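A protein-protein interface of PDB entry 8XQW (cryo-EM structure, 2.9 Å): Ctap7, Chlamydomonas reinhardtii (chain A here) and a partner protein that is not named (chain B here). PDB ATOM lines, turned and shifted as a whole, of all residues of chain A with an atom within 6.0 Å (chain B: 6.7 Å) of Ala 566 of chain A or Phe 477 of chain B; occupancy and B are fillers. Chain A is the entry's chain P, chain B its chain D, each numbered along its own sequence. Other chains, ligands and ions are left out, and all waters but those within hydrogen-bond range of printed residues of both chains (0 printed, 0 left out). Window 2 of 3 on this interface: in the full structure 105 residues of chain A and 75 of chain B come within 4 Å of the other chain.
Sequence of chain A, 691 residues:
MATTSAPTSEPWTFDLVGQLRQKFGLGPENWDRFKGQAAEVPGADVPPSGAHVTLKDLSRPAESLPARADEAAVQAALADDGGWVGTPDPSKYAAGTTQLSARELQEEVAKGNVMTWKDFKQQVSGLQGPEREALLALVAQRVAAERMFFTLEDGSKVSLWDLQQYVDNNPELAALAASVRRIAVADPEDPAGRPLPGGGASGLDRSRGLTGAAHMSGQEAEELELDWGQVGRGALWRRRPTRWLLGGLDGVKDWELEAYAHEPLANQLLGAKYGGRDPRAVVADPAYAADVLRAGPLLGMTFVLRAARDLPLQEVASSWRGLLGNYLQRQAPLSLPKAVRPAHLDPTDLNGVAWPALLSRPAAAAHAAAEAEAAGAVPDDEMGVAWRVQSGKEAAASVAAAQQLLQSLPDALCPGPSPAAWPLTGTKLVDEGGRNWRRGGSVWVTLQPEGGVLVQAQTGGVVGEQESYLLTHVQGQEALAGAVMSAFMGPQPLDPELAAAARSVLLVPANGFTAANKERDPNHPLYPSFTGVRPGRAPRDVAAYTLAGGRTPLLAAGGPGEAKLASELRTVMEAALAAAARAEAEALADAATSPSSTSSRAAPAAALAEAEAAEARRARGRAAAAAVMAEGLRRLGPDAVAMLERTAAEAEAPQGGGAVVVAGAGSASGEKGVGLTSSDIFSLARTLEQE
Printed residues of chain B within 4 Å of Glu 562 of chain A: Leu 476 (3.1 Å). Ala 563 of chain A touches none of the printed residues of chain B. Ala 566 of chain A touches just one residue of chain B: Phe 477 (3.4 Å). Printed residues of chain B within 4 Å of Arg 570 of chain A: Phe 477 (2.8 Å) and Ser 478 (3.9 Å). Of the printed residues of chain B, Thr 647 of chain A touches Phe 477 (3.7 Å). Printed residues of chain A within 4 Å of Leu 476 of chain B: Glu 562 (3.1 Å). Phe 477 of chain B touches five residues of chain A. Printed residues of chain A within 4 Å of Ser 478 of chain B: Arg 570 (3.9 Å). The nearest residue of chain B that does not touch Ala 566 of chain A is Leu 476 of chain B (4.3 Å).
Hydrophobic or aromatic side chains of chain A that line the printed part of chain B: Ala 566, Leu 569 and Met 573. Along chain A the printed residues that touch a printed residue of chain B span positions 562 to 647. Among the printed residues, 7 pairs touch across the chains.
Among the printed residues, merely in contact across the chains: Glu 562 of chain A with Leu 476 of chain B, Ala 566 of chain A with Phe 477 of chain B, Met 573 of chain A with Phe 477 of chain B, Leu 569 of chain A with Phe 477 of chain B, Thr 647 of chain A with Phe 477 of chain B and Arg 570 of chain A with Ser 478 of chain B.
The guanidinium group (NH1) of Arg 570 of chain A is in hydrogen-bond range of the backbone carbonyl oxygen (O) of Phe 477 of chain B, 2.8 Å away.
The backbone carbonyl oxygen of Met 643 of chain A is in hydrogen-bond range of the side-chain hydroxyl of Thr 647 of chain A, at 2.8 Å.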
ATOM      1  N   GLY A 561       5.627  -8.162  -0.156  1.00  0.00           N
ATOM      2  CA  GLY A 561       6.035  -6.899  -0.743  1.00  0.00           C
ATOM      3  C   GLY A 561       5.229  -5.717  -0.252  1.00  0.00           C
ATOM      4  O   GLY A 561       5.791  -4.647   0.010  1.00  0.00           O
ATOM      5  N   GLU A 562       3.911  -5.889  -0.126  1.00  0.00           N
ATOM      6  CA  GLU A 562       3.068  -4.845   0.440  1.00  0.00           C
ATOM      7  C   GLU A 562       3.497  -4.483   1.857  1.00  0.00           C
ATOM      8  O   GLU A 562       3.390  -3.318   2.259  1.00  0.00           O
ATOM      9  CB  GLU A 562       1.610  -5.299   0.416  1.00  0.00           C
ATOM     10  CG  GLU A 562       0.640  -4.358   1.105  1.00  0.00           C
ATOM     11  CD  GLU A 562       0.355  -4.756   2.538  1.00  0.00           C
ATOM     12  OE1 GLU A 562       0.937  -4.140   3.453  1.00  0.00           O
ATOM     13  OE2 GLU A 562      -0.455  -5.682   2.748  1.00  0.00           O
ATOM     14  N   ALA A 563       4.002  -5.458   2.615  1.00  0.00           N
ATOM     15  CA  ALA A 563       4.428  -5.195   3.985  1.00  0.00           C
ATOM     16  C   ALA A 563       5.589  -4.210   4.023  1.00  0.00           C
ATOM     17  O   ALA A 563       5.527  -3.190   4.718  1.00  0.00           O
ATOM     18  CB  ALA A 563       4.810  -6.502   4.674  1.00  0.00           C
ATOM     19  N   LYS A 564       6.658  -4.491   3.276  1.00  0.00           N
ATOM     20  CA  LYS A 564       7.783  -3.564   3.255  1.00  0.00           C
ATOM     21  C   LYS A 564       7.408  -2.247   2.589  1.00  0.00           C
ATOM     22  O   LYS A 564       7.935  -1.194   2.969  1.00  0.00           O
ATOM     23  CB  LYS A 564       8.985  -4.202   2.557  1.00  0.00           C
ATOM     24  CG  LYS A 564       8.668  -4.868   1.233  1.00  0.00           C
ATOM     25  CD  LYS A 564       9.102  -4.008   0.060  1.00  0.00           C
ATOM     26  CE  LYS A 564       8.855  -4.719  -1.259  1.00  0.00           C
ATOM     27  NZ  LYS A 564       9.469  -4.006  -2.411  1.00  0.00           N
ATOM     28  N   LEU A 565       6.511  -2.282   1.599  1.00  0.00           N
ATOM     29  CA  LEU A 565       5.999  -1.045   1.019  1.00  0.00           C
ATOM     30  C   LEU A 565       5.423  -0.144   2.101  1.00  0.00           C
ATOM     31  O   LEU A 565       5.844   1.011   2.263  1.00  0.00           O
ATOM     32  CB  LEU A 565       4.941  -1.377  -0.036  1.00  0.00           C
ATOM     33  CG  LEU A 565       4.574  -0.401  -1.164  1.00  0.00           C
ATOM     34  CD1 LEU A 565       3.936   0.882  -0.638  1.00  0.00           C
ATOM     35  CD2 LEU A 565       5.777  -0.090  -2.046  1.00  0.00           C
ATOM     36  N   ALA A 566       4.442  -0.664   2.845  1.00  0.00           N
ATOM     37  CA  ALA A 566       3.863   0.075   3.958  1.00  0.00           C
ATOM     38  C   ALA A 566       4.922   0.465   4.978  1.00  0.00           C
ATOM     39  O   ALA A 566       4.817   1.525   5.594  1.00  0.00           O
ATOM     40  CB  ALA A 566       2.766  -0.752   4.622  1.00  0.00           C
ATOM     41  N   SER A 567       5.961  -0.356   5.142  1.00  0.00           N
ATOM     42  CA  SER A 567       7.015  -0.039   6.101  1.00  0.00           C
ATOM     43  C   SER A 567       7.775   1.226   5.718  1.00  0.00           C
ATOM     44  O   SER A 567       7.881   2.163   6.523  1.00  0.00           O
ATOM     45  CB  SER A 567       7.979  -1.216   6.221  1.00  0.00           C
ATOM     46  OG  SER A 567       9.299  -0.757   6.451  1.00  0.00           O
ATOM     47  N   GLU A 568       8.330   1.268   4.503  1.00  0.00           N
ATOM     48  CA  GLU A 568       9.087   2.454   4.113  1.00  0.00           C
ATOM     49  C   GLU A 568       8.181   3.676   3.993  1.00  0.00           C
ATOM     50  O   GLU A 568       8.575   4.791   4.370  1.00  0.00           O
ATOM     51  CB  GLU A 568       9.873   2.238   2.813  1.00  0.00           C
ATOM     52  CG  GLU A 568       9.145   1.612   1.636  1.00  0.00           C
ATOM     53  CD  GLU A 568       9.646   0.215   1.327  1.00  0.00           C
ATOM     54  OE1 GLU A 568      10.588  -0.238   2.011  1.00  0.00           O
ATOM     55  OE2 GLU A 568       9.098  -0.435   0.412  1.00  0.00           O
ATOM     56  N   LEU A 569       6.955   3.495   3.490  1.00  0.00           N
ATOM     57  CA  LEU A 569       6.072   4.651   3.384  1.00  0.00           C
ATOM     58  C   LEU A 569       5.672   5.161   4.762  1.00  0.00           C
ATOM     59  O   LEU A 569       5.545   6.376   4.966  1.00  0.00           O
ATOM     60  CB  LEU A 569       4.845   4.307   2.536  1.00  0.00           C
ATOM     61  CG  LEU A 569       3.744   5.355   2.342  1.00  0.00           C
ATOM     62  CD1 LEU A 569       3.123   5.172   0.979  1.00  0.00           C
ATOM     63  CD2 LEU A 569       2.671   5.218   3.394  1.00  0.00           C
ATOM     64  N   ARG A 570       5.513   4.260   5.731  1.00  0.00           N
ATOM     65  CA  ARG A 570       5.220   4.674   7.094  1.00  0.00           C
ATOM     66  C   ARG A 570       6.396   5.421   7.699  1.00  0.00           C
ATOM     67  O   ARG A 570       6.205   6.427   8.385  1.00  0.00           O
ATOM     68  CB  ARG A 570       4.855   3.451   7.930  1.00  0.00           C
ATOM     69  CG  ARG A 570       5.056   3.599   9.426  1.00  0.00           C
ATOM     70  CD  ARG A 570       5.227   2.224  10.051  1.00  0.00           C
ATOM     71  NE  ARG A 570       5.272   2.264  11.507  1.00  0.00           N
ATOM     72  CZ  ARG A 570       5.367   1.185  12.279  1.00  0.00           C
ATOM     73  NH1 ARG A 570       5.428  -0.020  11.730  1.00  0.00           N
ATOM     74  NH2 ARG A 570       5.399   1.309  13.597  1.00  0.00           N
ATOM     75  N   THR A 571       7.618   4.946   7.453  1.00  0.00           N
ATOM     76  CA  THR A 571       8.800   5.658   7.933  1.00  0.00           C
ATOM     77  C   THR A 571       8.828   7.086   7.402  1.00  0.00           C
ATOM     78  O   THR A 571       9.062   8.047   8.153  1.00  0.00           O
ATOM     79  CB  THR A 571      10.063   4.911   7.508  1.00  0.00           C
ATOM     80  OG1 THR A 571       9.800   3.503   7.489  1.00  0.00           O
ATOM     81  CG2 THR A 571      11.204   5.199   8.470  1.00  0.00           C
ATOM     82  N   MET A 573       6.330   8.936   6.248  1.00  0.00           N
ATOM     83  CA  MET A 573       5.285   9.816   6.773  1.00  0.00           C
ATOM     84  C   MET A 573       5.508  10.103   8.255  1.00  0.00           C
ATOM     85  O   MET A 573       5.029  11.114   8.775  1.00  0.00           O
ATOM     86  CB  MET A 573       3.877   9.259   6.546  1.00  0.00           C
ATOM     87  CG  MET A 573       3.650   7.797   6.776  1.00  0.00           C
ATOM     88  SD  MET A 573       2.046   7.347   6.084  1.00  0.00           S
ATOM     89  CE  MET A 573       1.536   6.037   7.191  1.00  0.00           C
ATOM     90  N   MET A 643      -1.134   2.808  -2.593  1.00  0.00           N
ATOM     91  CA  MET A 643      -1.366   2.411  -1.210  1.00  0.00           C
ATOM     92  C   MET A 643      -1.884   3.577  -0.382  1.00  0.00           C
ATOM     93  O   MET A 643      -2.864   3.435   0.361  1.00  0.00           O
ATOM     94  CB  MET A 643      -0.079   1.861  -0.603  1.00  0.00           C
ATOM     95  CG  MET A 643      -0.220   1.387   0.831  1.00  0.00           C
ATOM     96  SD  MET A 643      -1.786   0.561   1.153  1.00  0.00           S
ATOM     97  CE  MET A 643      -1.235  -1.139   1.292  1.00  0.00           C
ATOM     98  N   THR A 647      -5.602   3.833   1.338  1.00  0.00           N
ATOM     99  CA  THR A 647      -5.764   4.018   2.777  1.00  0.00           C
ATOM    100  C   THR A 647      -6.562   5.277   3.077  1.00  0.00           C
ATOM    101  O   THR A 647      -7.422   5.283   3.968  1.00  0.00           O
ATOM    102  CB  THR A 647      -4.397   4.078   3.455  1.00  0.00           C
ATOM    103  OG1 THR A 647      -3.505   4.850   2.648  1.00  0.00           O
ATOM    104  CG2 THR A 647      -3.831   2.673   3.660  1.00  0.00           C
ATOM    105  N   ILE A 681      -3.237   9.922   8.971  1.00  0.00           N
ATOM    106  CA  ILE A 681      -2.887   9.564   7.601  1.00  0.00           C
ATOM    107  C   ILE A 681      -3.843  10.205   6.601  1.00  0.00           C
ATOM    108  O   ILE A 681      -3.423  10.665   5.535  1.00  0.00           O
ATOM    109  CB  ILE A 681      -2.817   8.036   7.446  1.00  0.00           C
ATOM    110  CG1 ILE A 681      -2.474   7.662   6.005  1.00  0.00           C
ATOM    111  CG2 ILE A 681      -4.112   7.385   7.870  1.00  0.00           C
ATOM    112  CD1 ILE A 681      -2.465   6.177   5.757  1.00  0.00           C
ATOM    113  N   LYS B 472      -7.861  -3.162   9.769  1.00  0.00           N
ATOM    114  CA  LYS B 472      -6.811  -4.045   9.275  1.00  0.00           C
ATOM    115  C   LYS B 472      -5.634  -3.253   8.719  1.00  0.00           C
ATOM    116  O   LYS B 472      -4.479  -3.530   9.056  1.00  0.00           O
ATOM    117  CB  LYS B 472      -7.377  -4.990   8.219  1.00  0.00           C
ATOM    118  CG  LYS B 472      -6.545  -6.243   7.986  1.00  0.00           C
ATOM    119  CD  LYS B 472      -5.425  -5.987   6.994  1.00  0.00           C
ATOM    120  CE  LYS B 472      -4.969  -7.262   6.320  1.00  0.00           C
ATOM    121  NZ  LYS B 472      -4.325  -6.958   5.017  1.00  0.00           N
ATOM    122  N   ASN B 473      -5.903  -2.263   7.867  1.00  0.00           N
ATOM    123  CA  ASN B 473      -4.811  -1.522   7.243  1.00  0.00           C
ATOM    124  C   ASN B 473      -4.051  -0.676   8.256  1.00  0.00           C
ATOM    125  O   ASN B 473      -2.815  -0.622   8.228  1.00  0.00           O
ATOM    126  CB  ASN B 473      -5.341  -0.658   6.101  1.00  0.00           C
ATOM    127  CG  ASN B 473      -5.843  -1.482   4.940  1.00  0.00           C
ATOM    128  OD1 ASN B 473      -6.701  -2.345   5.101  1.00  0.00           O
ATOM    129  ND2 ASN B 473      -5.294  -1.230   3.760  1.00  0.00           N
ATOM    130  N   LEU B 474      -4.767  -0.006   9.164  1.00  0.00           N
ATOM    131  CA  LEU B 474      -4.067   0.828  10.138  1.00  0.00           C
ATOM    132  C   LEU B 474      -3.275  -0.026  11.120  1.00  0.00           C
ATOM    133  O   LEU B 474      -2.231   0.404  11.622  1.00  0.00           O
ATOM    134  CB  LEU B 474      -5.057   1.739  10.866  1.00  0.00           C
ATOM    135  CG  LEU B 474      -5.845   1.256  12.087  1.00  0.00           C
ATOM    136  CD1 LEU B 474      -5.093   1.512  13.394  1.00  0.00           C
ATOM    137  CD2 LEU B 474      -7.214   1.915  12.112  1.00  0.00           C
ATOM    138  N   PHE B 475      -3.750  -1.242  11.403  1.00  0.00           N
ATOM    139  CA  PHE B 475      -2.976  -2.162  12.228  1.00  0.00           C
ATOM    140  C   PHE B 475      -1.741  -2.651  11.487  1.00  0.00           C
ATOM    141  O   PHE B 475      -0.672  -2.813  12.086  1.00  0.00           O
ATOM    142  CB  PHE B 475      -3.848  -3.343  12.649  1.00  0.00           C
ATOM    143  CG  PHE B 475      -3.143  -4.669  12.597  1.00  0.00           C
ATOM    144  CD1 PHE B 475      -2.257  -5.037  13.594  1.00  0.00           C
ATOM    145  CD2 PHE B 475      -3.362  -5.544  11.544  1.00  0.00           C
ATOM    146  CE1 PHE B 475      -1.602  -6.252  13.546  1.00  0.00           C
ATOM    147  CE2 PHE B 475      -2.711  -6.760  11.490  1.00  0.00           C
ATOM    148  CZ  PHE B 475      -1.829  -7.115  12.491  1.00  0.00           C
ATOM    149  N   LEU B 476      -1.874  -2.906  10.185  1.00  0.00           N
ATOM    150  CA  LEU B 476      -0.722  -3.327   9.400  1.00  0.00           C
ATOM    151  C   LEU B 476       0.328  -2.227   9.339  1.00  0.00           C
ATOM    152  O   LEU B 476       1.529  -2.511   9.352  1.00  0.00           O
ATOM    153  CB  LEU B 476      -1.163  -3.732   7.992  1.00  0.00           C
ATOM    154  CG  LEU B 476      -0.281  -4.740   7.248  1.00  0.00           C
ATOM    155  CD1 LEU B 476       0.916  -4.075   6.586  1.00  0.00           C
ATOM    156  CD2 LEU B 476       0.172  -5.840   8.194  1.00  0.00           C
ATOM    157  N   PHE B 477      -0.106  -0.968   9.276  1.00  0.00           N
ATOM    158  CA  PHE B 477       0.844   0.138   9.316  1.00  0.00           C
ATOM    159  C   PHE B 477       1.542   0.202  10.667  1.00  0.00           C
ATOM    160  O   PHE B 477       2.775   0.212  10.746  1.00  0.00           O
ATOM    161  CB  PHE B 477       0.134   1.457   9.011  1.00  0.00           C
ATOM    162  CG  PHE B 477       0.308   1.919   7.598  1.00  0.00           C
ATOM    163  CD1 PHE B 477       1.531   2.391   7.158  1.00  0.00           C
ATOM    164  CD2 PHE B 477      -0.752   1.888   6.712  1.00  0.00           C
ATOM    165  CE1 PHE B 477       1.694   2.813   5.857  1.00  0.00           C
ATOM    166  CE2 PHE B 477      -0.595   2.313   5.410  1.00  0.00           C
ATOM    167  CZ  PHE B 477       0.630   2.778   4.982  1.00  0.00           C
ATOM    168  N   SER B 478       0.766   0.241  11.745  1.00  0.00           N
ATOM    169  CA  SER B 478       1.318   0.272  13.095  1.00  0.00           C
ATOM    170  C   SER B 478       1.803  -1.105  13.528  1.00  0.00           C
ATOM    171  O   SER B 478       2.154  -1.941  12.696  1.00  0.00           O
ATOM    172  CB  SER B 478       0.279   0.792  14.087  1.00  0.00           C
ATOM    173  OG  SER B 478       0.714   0.608  15.421  1.00  0.00           O
